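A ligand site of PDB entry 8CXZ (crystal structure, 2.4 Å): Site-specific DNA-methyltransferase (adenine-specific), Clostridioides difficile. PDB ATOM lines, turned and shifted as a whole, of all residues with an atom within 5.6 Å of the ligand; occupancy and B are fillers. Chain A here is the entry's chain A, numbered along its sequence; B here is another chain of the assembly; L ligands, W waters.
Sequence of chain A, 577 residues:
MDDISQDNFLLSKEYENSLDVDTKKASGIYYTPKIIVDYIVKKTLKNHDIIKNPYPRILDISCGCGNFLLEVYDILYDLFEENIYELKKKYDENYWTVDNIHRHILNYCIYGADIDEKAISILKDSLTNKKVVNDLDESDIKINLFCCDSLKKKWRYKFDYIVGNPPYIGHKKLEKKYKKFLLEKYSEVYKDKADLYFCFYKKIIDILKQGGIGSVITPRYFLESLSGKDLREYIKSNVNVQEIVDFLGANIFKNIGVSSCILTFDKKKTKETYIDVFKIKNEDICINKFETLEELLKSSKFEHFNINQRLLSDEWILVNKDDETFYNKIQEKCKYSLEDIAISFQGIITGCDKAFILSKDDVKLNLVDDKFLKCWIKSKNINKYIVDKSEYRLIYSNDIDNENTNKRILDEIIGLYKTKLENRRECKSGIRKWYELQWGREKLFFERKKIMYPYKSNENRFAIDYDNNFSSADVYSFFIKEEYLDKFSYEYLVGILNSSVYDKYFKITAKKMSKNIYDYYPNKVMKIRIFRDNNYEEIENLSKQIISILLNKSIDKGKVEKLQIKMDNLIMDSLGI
An oxygen (O1) of the ligand lies within hydrogen-bond range of the side-chain carboxylate (OD1) of Asp 114 (2.5 Å). A nitrogen (N5) of the ligand sits at hydrogen-bond distance from the side-chain carboxylate of Asp 149, 2.7 Å away. The backbone NH (N) of Ser 150 sits at hydrogen-bond distance from a nitrogen (N4) of the ligand (2.9 Å). The backbone NH (N) of Ile 115 sits at hydrogen-bond distance from a nitrogen (N3) of the ligand, 3.3 Å away.
The backbone NH (N) of Asp 116 sits at hydrogen-bond distance from the side-chain carboxylate (OD1) of Asp 114 (2.9 Å). OD2 of Asp 149 sits at hydrogen-bond distance from OH of Tyr 178, at 2.6 Å. N of Leu 151 lies within hydrogen-bond range of OD1 of Asp 149, 2.9 Å away. OG of Ser 150 is in hydrogen-bond range of O of Ile 61, 2.6 Å away. OG of Ser 62 lies within hydrogen-bond range of O of Asn 165 (2.9 Å). O of Cys 148 lies close to N of Ile 115, 3.5 Å away. N1 of DA 8 of chain B lies within hydrogen-bond range of the side-chain amide nitrogen of Asn 165 (3.0 Å). The backbone NH (N) of Ala 119 sits at hydrogen-bond distance from the side-chain carboxylate (OD2) of Asp 116 (3.4 Å).
Merely in contact with the ligand: Ser 62 (3.2 Å), Pro 167 (3.4 Å), Tyr 178 (3.5 Å), Gly 28 (3.5 Å), Phe 200 (3.6 Å), Tyr 30 (3.6 Å), Glu 175 (3.6 Å), Cys 148 (3.7 Å), Gly 64 (3.7 Å), Ile 61 (3.7 Å), DA 8 of chain B (3.8 Å), Asn 165 (3.9 Å) and Asp 116 (3.96 Å). The nearest printed residue that does not touch the ligand is Leu 196 (4.01 Å).
Water W1 bridges N7 of DA 8 of chain B (3.2 Å) and an oxygen (O2) of the ligand (3.4 Å).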
ATOM      1  N   GLY A  28      19.854   9.995  24.602  1.00  0.00           N
ATOM      2  CA  GLY A  28      19.841   8.574  24.868  1.00  0.00           C
ATOM      3  C   GLY A  28      18.767   7.809  24.115  1.00  0.00           C
ATOM      4  O   GLY A  28      18.997   7.321  23.010  1.00  0.00           O
ATOM      5  N   ILE A  29      17.583   7.705  24.726  1.00  0.00           N
ATOM      6  CA  ILE A  29      16.481   6.921  24.179  1.00  0.00           C
ATOM      7  C   ILE A  29      15.295   7.840  23.916  1.00  0.00           C
ATOM      8  O   ILE A  29      14.964   8.703  24.745  1.00  0.00           O
ATOM      9  CB  ILE A  29      16.068   5.772  25.132  1.00  0.00           C
ATOM     10  N   TYR A  30      14.661   7.651  22.760  1.00  0.00           N
ATOM     11  CA  TYR A  30      13.569   8.495  22.293  1.00  0.00           C
ATOM     12  C   TYR A  30      12.258   7.712  22.272  1.00  0.00           C
ATOM     13  O   TYR A  30      12.228   6.554  21.853  1.00  0.00           O
ATOM     14  CB  TYR A  30      13.867   9.059  20.903  1.00  0.00           C
ATOM     15  CG  TYR A  30      15.126   9.892  20.839  1.00  0.00           C
ATOM     16  CD1 TYR A  30      16.359   9.305  20.597  1.00  0.00           C
ATOM     17  CD2 TYR A  30      15.074  11.266  21.006  1.00  0.00           C
ATOM     18  CE1 TYR A  30      17.513  10.058  20.533  1.00  0.00           C
ATOM     19  CE2 TYR A  30      16.217  12.038  20.946  1.00  0.00           C
ATOM     20  CZ  TYR A  30      17.438  11.432  20.705  1.00  0.00           C
ATOM     21  OH  TYR A  30      18.572  12.199  20.644  1.00  0.00           O
ATOM     22  N   ILE A  61      15.376  -3.657  16.000  1.00  0.00           N
ATOM     23  CA  ILE A  61      16.839  -3.614  16.006  1.00  0.00           C
ATOM     24  C   ILE A  61      17.388  -2.490  16.873  1.00  0.00           C
ATOM     25  O   ILE A  61      18.583  -2.497  17.200  1.00  0.00           O
ATOM     26  CB  ILE A  61      17.264  -3.568  14.518  1.00  0.00           C
ATOM     27  CG1 ILE A  61      17.631  -4.972  14.035  1.00  0.00           C
ATOM     28  CG2 ILE A  61      18.394  -2.609  14.261  1.00  0.00           C
ATOM     29  CD1 ILE A  61      17.943  -5.038  12.573  1.00  0.00           C
ATOM     30  N   SER A  62      16.554  -1.548  17.290  1.00  0.00           N
ATOM     31  CA  SER A  62      16.872  -0.513  18.265  1.00  0.00           C
ATOM     32  C   SER A  62      15.748  -0.413  19.290  1.00  0.00           C
ATOM     33  O   SER A  62      15.168   0.653  19.524  1.00  0.00           O
ATOM     34  CB  SER A  62      17.154   0.820  17.579  1.00  0.00           C
ATOM     35  OG  SER A  62      16.108   1.176  16.706  1.00  0.00           O
ATOM     36  N   CYS A  63      15.394  -1.558  19.869  1.00  0.00           N
ATOM     37  CA  CYS A  63      14.144  -1.700  20.617  1.00  0.00           C
ATOM     38  C   CYS A  63      14.067  -0.846  21.866  1.00  0.00           C
ATOM     39  O   CYS A  63      12.958  -0.593  22.361  1.00  0.00           O
ATOM     40  CB  CYS A  63      13.943  -3.162  20.992  1.00  0.00           C
ATOM     41  SG  CYS A  63      15.246  -3.824  22.061  1.00  0.00           S
ATOM     42  N   GLY A  64      15.201  -0.399  22.413  1.00  0.00           N
ATOM     43  CA  GLY A  64      15.155   0.432  23.612  1.00  0.00           C
ATOM     44  C   GLY A  64      14.494  -0.314  24.760  1.00  0.00           C
ATOM     45  O   GLY A  64      14.818  -1.461  25.055  1.00  0.00           O
ATOM     46  N   ALA A 113      17.146  -6.005  19.803  1.00  0.00           N
ATOM     47  CA  ALA A 113      18.546  -5.664  19.954  1.00  0.00           C
ATOM     48  C   ALA A 113      18.653  -4.187  20.318  1.00  0.00           C
ATOM     49  O   ALA A 113      17.900  -3.355  19.801  1.00  0.00           O
ATOM     50  CB  ALA A 113      19.341  -5.942  18.673  1.00  0.00           C
ATOM     51  N   ASP A 114      19.577  -3.878  21.219  1.00  0.00           N
ATOM     52  CA  ASP A 114      19.855  -2.486  21.547  1.00  0.00           C
ATOM     53  C   ASP A 114      21.238  -2.381  22.160  1.00  0.00           C
ATOM     54  O   ASP A 114      21.732  -3.315  22.791  1.00  0.00           O
ATOM     55  CB  ASP A 114      18.809  -1.905  22.507  1.00  0.00           C
ATOM     56  CG  ASP A 114      18.783  -0.390  22.485  1.00  0.00           C
ATOM     57  OD1 ASP A 114      19.734   0.236  23.015  1.00  0.00           O
ATOM     58  OD2 ASP A 114      17.825   0.185  21.916  1.00  0.00           O
ATOM     59  N   ILE A 115      21.857  -1.217  21.957  1.00  0.00           N
ATOM     60  CA  ILE A 115      23.216  -0.985  22.455  1.00  0.00           C
ATOM     61  C   ILE A 115      23.236  -0.760  23.968  1.00  0.00           C
ATOM     62  O   ILE A 115      24.285  -0.924  24.593  1.00  0.00           O
ATOM     63  CB  ILE A 115      23.831   0.211  21.710  1.00  0.00           C
ATOM     64  CG1 ILE A 115      25.349   0.198  21.813  1.00  0.00           C
ATOM     65  CG2 ILE A 115      23.263   1.532  22.233  1.00  0.00           C
ATOM     66  CD1 ILE A 115      25.991  -0.884  21.000  1.00  0.00           C
ATOM     67  N   ASP A 116      22.096  -0.417  24.574  1.00  0.00           N
ATOM     68  CA  ASP A 116      22.018   0.002  25.971  1.00  0.00           C
ATOM     69  C   ASP A 116      21.533  -1.160  26.825  1.00  0.00           C
ATOM     70  O   ASP A 116      20.368  -1.574  26.715  1.00  0.00           O
ATOM     71  CB  ASP A 116      21.098   1.217  26.103  1.00  0.00           C
ATOM     72  CG  ASP A 116      20.850   1.618  27.546  1.00  0.00           C
ATOM     73  OD1 ASP A 116      21.747   1.385  28.390  1.00  0.00           O
ATOM     74  OD2 ASP A 116      19.765   2.158  27.834  1.00  0.00           O
ATOM     75  N   ALA A 119      18.368  -0.661  29.052  1.00  0.00           N
ATOM     76  CA  ALA A 119      17.100  -0.783  28.345  1.00  0.00           C
ATOM     77  C   ALA A 119      16.722  -2.245  28.111  1.00  0.00           C
ATOM     78  O   ALA A 119      15.558  -2.619  28.265  1.00  0.00           O
ATOM     79  CB  ALA A 119      17.171  -0.024  27.018  1.00  0.00           C
ATOM     80  N   CYS A 148      23.931  -5.318  21.986  1.00  0.00           N
ATOM     81  CA  CYS A 148      24.985  -5.320  20.976  1.00  0.00           C
ATOM     82  C   CYS A 148      24.767  -4.135  20.050  1.00  0.00           C
ATOM     83  O   CYS A 148      23.727  -3.469  20.072  1.00  0.00           O
ATOM     84  CB  CYS A 148      24.972  -6.620  20.171  1.00  0.00           C
ATOM     85  SG  CYS A 148      23.530  -6.732  19.062  1.00  0.00           S
ATOM     86  N   ASP A 149      25.775  -3.878  19.220  1.00  0.00           N
ATOM     87  CA  ASP A 149      25.659  -2.963  18.098  1.00  0.00           C
ATOM     88  C   ASP A 149      24.973  -3.707  16.955  1.00  0.00           C
ATOM     89  O   ASP A 149      25.560  -4.625  16.368  1.00  0.00           O
ATOM     90  CB  ASP A 149      27.039  -2.440  17.685  1.00  0.00           C
ATOM     91  CG  ASP A 149      26.990  -1.436  16.542  1.00  0.00           C
ATOM     92  OD1 ASP A 149      25.912  -1.246  15.935  1.00  0.00           O
ATOM     93  OD2 ASP A 149      28.051  -0.849  16.236  1.00  0.00           O
ATOM     94  N   SER A 150      23.740  -3.316  16.637  1.00  0.00           N
ATOM     95  CA  SER A 150      22.984  -4.026  15.606  1.00  0.00           C
ATOM     96  C   SER A 150      23.648  -3.955  14.235  1.00  0.00           C
ATOM     97  O   SER A 150      23.395  -4.815  13.399  1.00  0.00           O
ATOM     98  CB  SER A 150      21.562  -3.481  15.526  1.00  0.00           C
ATOM     99  OG  SER A 150      20.850  -3.729  16.721  1.00  0.00           O
ATOM    100  N   LEU A 151      24.492  -2.952  14.003  1.00  0.00           N
ATOM    101  CA  LEU A 151      25.181  -2.826  12.722  1.00  0.00           C
ATOM    102  C   LEU A 151      26.395  -3.732  12.622  1.00  0.00           C
ATOM    103  O   LEU A 151      26.930  -3.902  11.519  1.00  0.00           O
ATOM    104  CB  LEU A 151      25.590  -1.373  12.484  1.00  0.00           C
ATOM    105  CG  LEU A 151      24.452  -0.361  12.424  1.00  0.00           C
ATOM    106  CD1 LEU A 151      24.963   1.007  11.976  1.00  0.00           C
ATOM    107  CD2 LEU A 151      23.334  -0.851  11.501  1.00  0.00           C
ATOM    108  N   ASN A 165      12.150   2.253  15.594  1.00  0.00           N
ATOM    109  CA  ASN A 165      12.596   3.634  15.400  1.00  0.00           C
ATOM    110  C   ASN A 165      14.112   3.663  15.599  1.00  0.00           C
ATOM    111  O   ASN A 165      14.592   3.638  16.750  1.00  0.00           O
ATOM    112  CB  ASN A 165      11.899   4.574  16.375  1.00  0.00           C
ATOM    113  CG  ASN A 165      12.362   6.010  16.248  1.00  0.00           C
ATOM    114  OD1 ASN A 165      12.917   6.408  15.226  1.00  0.00           O
ATOM    115  ND2 ASN A 165      12.155   6.789  17.302  1.00  0.00           N
ATOM    116  N   PRO A 166      14.883   3.722  14.519  1.00  0.00           N
ATOM    117  CA  PRO A 166      16.345   3.624  14.636  1.00  0.00           C
ATOM    118  C   PRO A 166      16.945   4.909  15.191  1.00  0.00           C
ATOM    119  O   PRO A 166      16.257   5.927  15.314  1.00  0.00           O
ATOM    120  CB  PRO A 166      16.796   3.397  13.177  1.00  0.00           C
ATOM    121  CG  PRO A 166      15.753   4.112  12.381  1.00  0.00           C
ATOM    122  CD  PRO A 166      14.446   3.890  13.121  1.00  0.00           C
ATOM    123  N   PRO A 167      18.223   4.890  15.561  1.00  0.00           N
ATOM    124  CA  PRO A 167      18.885   6.145  15.959  1.00  0.00           C
ATOM    125  C   PRO A 167      19.179   7.015  14.748  1.00  0.00           C
ATOM    126  O   PRO A 167      19.493   6.520  13.665  1.00  0.00           O
ATOM    127  CB  PRO A 167      20.184   5.663  16.614  1.00  0.00           C
ATOM    128  CG  PRO A 167      20.452   4.344  15.975  1.00  0.00           C
ATOM    129  CD  PRO A 167      19.108   3.724  15.746  1.00  0.00           C
ATOM    130  N   ILE A 169      21.768   9.919  13.743  1.00  0.00           N
ATOM    131  CA  ILE A 169      22.988  10.644  14.099  1.00  0.00           C
ATOM    132  C   ILE A 169      23.633  11.147  12.817  1.00  0.00           C
ATOM    133  O   ILE A 169      23.980  10.347  11.938  1.00  0.00           O
ATOM    134  CB  ILE A 169      23.983   9.773  14.893  1.00  0.00           C
ATOM    135  CG1 ILE A 169      23.288   9.134  16.096  1.00  0.00           C
ATOM    136  CG2 ILE A 169      25.157  10.614  15.352  1.00  0.00           C
ATOM    137  CD1 ILE A 169      24.200   8.306  16.976  1.00  0.00           C
ATOM    138  N   LEU A 174      28.336  12.103  14.865  1.00  0.00           N
ATOM    139  CA  LEU A 174      28.762  10.714  14.834  1.00  0.00           C
ATOM    140  C   LEU A 174      30.266  10.617  15.066  1.00  0.00           C
ATOM    141  O   LEU A 174      31.034  11.375  14.466  1.00  0.00           O
ATOM    142  CB  LEU A 174      28.384  10.062  13.507  1.00  0.00           C
ATOM    143  CG  LEU A 174      28.583   8.540  13.405  1.00  0.00           C
ATOM    144  CD1 LEU A 174      27.938   7.839  14.590  1.00  0.00           C
ATOM    145  CD2 LEU A 174      27.996   8.021  12.105  1.00  0.00           C
ATOM    146  N   GLU A 175      30.672   9.702  15.933  1.00  0.00           N
ATOM    147  CA  GLU A 175      32.084   9.540  16.260  1.00  0.00           C
ATOM    148  C   GLU A 175      32.888   9.159  15.012  1.00  0.00           C
ATOM    149  O   GLU A 175      32.484   8.307  14.232  1.00  0.00           O
ATOM    150  CB  GLU A 175      32.249   8.471  17.339  1.00  0.00           C
ATOM    151  CG  GLU A 175      33.685   8.241  17.780  1.00  0.00           C
ATOM    152  CD  GLU A 175      33.790   7.209  18.890  1.00  0.00           C
ATOM    153  OE1 GLU A 175      32.760   6.601  19.228  1.00  0.00           O
ATOM    154  OE2 GLU A 175      34.910   7.025  19.411  1.00  0.00           O
ATOM    155  N   TYR A 178      33.895   5.477  14.497  1.00  0.00           N
ATOM    156  CA  TYR A 178      32.783   4.674  14.015  1.00  0.00           C
ATOM    157  C   TYR A 178      32.495   4.943  12.539  1.00  0.00           C
ATOM    158  O   TYR A 178      32.143   4.035  11.792  1.00  0.00           O
ATOM    159  CB  TYR A 178      31.542   4.936  14.864  1.00  0.00           C
ATOM    160  CG  TYR A 178      30.474   3.875  14.747  1.00  0.00           C
ATOM    161  CD1 TYR A 178      30.525   2.712  15.513  1.00  0.00           C
ATOM    162  CD2 TYR A 178      29.405   4.031  13.877  1.00  0.00           C
ATOM    163  CE1 TYR A 178      29.553   1.744  15.413  1.00  0.00           C
ATOM    164  CE2 TYR A 178      28.422   3.063  13.763  1.00  0.00           C
ATOM    165  CZ  TYR A 178      28.502   1.929  14.531  1.00  0.00           C
ATOM    166  OH  TYR A 178      27.530   0.960  14.430  1.00  0.00           O
ATOM    167  N   LEU A 196      23.398   8.031  10.123  1.00  0.00           N
ATOM    168  CA  LEU A 196      23.469   6.680  10.679  1.00  0.00           C
ATOM    169  C   LEU A 196      22.221   5.861  10.335  1.00  0.00           C
ATOM    170  O   LEU A 196      22.313   4.652  10.103  1.00  0.00           O
ATOM    171  CB  LEU A 196      23.641   6.763  12.194  1.00  0.00           C
ATOM    172  CG  LEU A 196      23.659   5.438  12.952  1.00  0.00           C
ATOM    173  CD1 LEU A 196      24.853   4.597  12.541  1.00  0.00           C
ATOM    174  CD2 LEU A 196      23.678   5.685  14.460  1.00  0.00           C
ATOM    175  N   PHE A 200      20.761   1.663   9.084  1.00  0.00           N
ATOM    176  CA  PHE A 200      19.706   0.825   9.660  1.00  0.00           C
ATOM    177  C   PHE A 200      18.685   0.415   8.609  1.00  0.00           C
ATOM    178  O   PHE A 200      18.198  -0.715   8.628  1.00  0.00           O
ATOM    179  CB  PHE A 200      19.043   1.540  10.834  1.00  0.00           C
ATOM    180  CG  PHE A 200      19.788   1.386  12.128  1.00  0.00           C
ATOM    181  CD1 PHE A 200      20.928   2.131  12.387  1.00  0.00           C
ATOM    182  CD2 PHE A 200      19.361   0.481  13.093  1.00  0.00           C
ATOM    183  CE1 PHE A 200      21.625   1.985  13.573  1.00  0.00           C
ATOM    184  CE2 PHE A 200      20.049   0.330  14.277  1.00  0.00           C
ATOM    185  CZ  PHE A 200      21.186   1.082  14.524  1.00  0.00           C
ATOM    186  P    DA B   8      20.391  16.688  13.538  1.00  0.00           P
ATOM    187  OP1  DA B   8      21.114  17.357  14.643  1.00  0.00           O
ATOM    188  OP2  DA B   8      21.018  15.544  12.848  1.00  0.00           O
ATOM    189  O5'  DA B   8      18.947  16.251  14.066  1.00  0.00           O
ATOM    190  C5'  DA B   8      18.765  14.999  14.688  1.00  0.00           C
ATOM    191  C4'  DA B   8      17.631  15.083  15.682  1.00  0.00           C
ATOM    192  O4'  DA B   8      16.929  13.815  15.738  1.00  0.00           O
ATOM    193  C3'  DA B   8      18.045  15.410  17.113  1.00  0.00           C
ATOM    194  O3'  DA B   8      17.098  16.314  17.667  1.00  0.00           O
ATOM    195  C2'  DA B   8      17.990  14.046  17.799  1.00  0.00           C
ATOM    196  C1'  DA B   8      16.789  13.428  17.091  1.00  0.00           C
ATOM    197  N9   DA B   8      16.753  11.974  17.148  1.00  0.00           N
ATOM    198  C8   DA B   8      17.813  11.110  17.065  1.00  0.00           C
ATOM    199  N7   DA B   8      17.470   9.838  17.137  1.00  0.00           N
ATOM    200  C5   DA B   8      16.095   9.874  17.264  1.00  0.00           C
ATOM    201  C6   DA B   8      15.121   8.858  17.382  1.00  0.00           C
ATOM    202  N6   DA B   8      15.420   7.558  17.397  1.00  0.00           N
ATOM    203  N1   DA B   8      13.825   9.224  17.484  1.00  0.00           N
ATOM    204  C2   DA B   8      13.528  10.539  17.477  1.00  0.00           C
ATOM    205  N3   DA B   8      14.354  11.586  17.369  1.00  0.00           N
ATOM    206  C4   DA B   8      15.630  11.175  17.271  1.00  0.00           C
HETATM  207  C1  LIG L   1      19.673   2.465  20.191  1.00  0.00           C
HETATM  208  C2  LIG L   1      21.727   3.361  19.020  1.00  0.00           C
HETATM  209  C3  LIG L   1      22.541   1.612  18.160  1.00  0.00           C
HETATM  210  C4  LIG L   1      17.093   4.833  19.530  1.00  0.00           C
HETATM  211  C5  LIG L   1      17.650   3.587  20.185  1.00  0.00           C
HETATM  212  C6  LIG L   1      19.746   3.387  21.401  1.00  0.00           C
HETATM  213  C7  LIG L   1      18.265   3.795  21.575  1.00  0.00           C
HETATM  214  O1  LIG L   1      20.236   2.672  22.522  1.00  0.00           O
HETATM  215  O2  LIG L   1      17.764   6.003  19.978  1.00  0.00           O
HETATM  216  N1  LIG L   1      20.912   2.348  19.428  1.00  0.00           N
HETATM  217  O3  LIG L   1      17.599   3.000  22.543  1.00  0.00           O
HETATM  218  C8  LIG L   1      24.822   2.116  16.294  1.00  0.00           C
HETATM  219  C9  LIG L   1      25.816   2.618  17.310  1.00  0.00           C
HETATM  220  C10 LIG L   1      26.281   4.044  17.038  1.00  0.00           C
HETATM  221  C11 LIG L   1      27.245   4.578  18.061  1.00  0.00           C
HETATM  222  C12 LIG L   1      28.614   4.555  17.836  1.00  0.00           C
HETATM  223  C13 LIG L   1      29.499   5.044  18.775  1.00  0.00           C
HETATM  224  C14 LIG L   1      29.026   5.570  19.960  1.00  0.00           C
HETATM  225  C15 LIG L   1      27.671   5.605  20.197  1.00  0.00           C
HETATM  226  C16 LIG L   1      26.787   5.116  19.258  1.00  0.00           C
HETATM  227  C17 LIG L   1      21.441   1.199  18.883  1.00  0.00           C
HETATM  228  C18 LIG L   1      21.738  -0.918  18.356  1.00  0.00           C
HETATM  229  C19 LIG L   1      23.252   0.584  17.468  1.00  0.00           C
HETATM  230  N2  LIG L   1      22.729   2.972  18.253  1.00  0.00           N
HETATM  231  N3  LIG L   1      20.983  -0.050  19.027  1.00  0.00           N
HETATM  232  N4  LIG L   1      22.822  -0.690  17.603  1.00  0.00           N
HETATM  233  N5  LIG L   1      24.289   0.810  16.641  1.00  0.00           N
HETATM  234  O4  LIG L   1      18.689   3.029  19.345  1.00  0.00           O
HETATM  235  O   HOH W   1      19.792   8.436  18.855  1.00  0.00           O
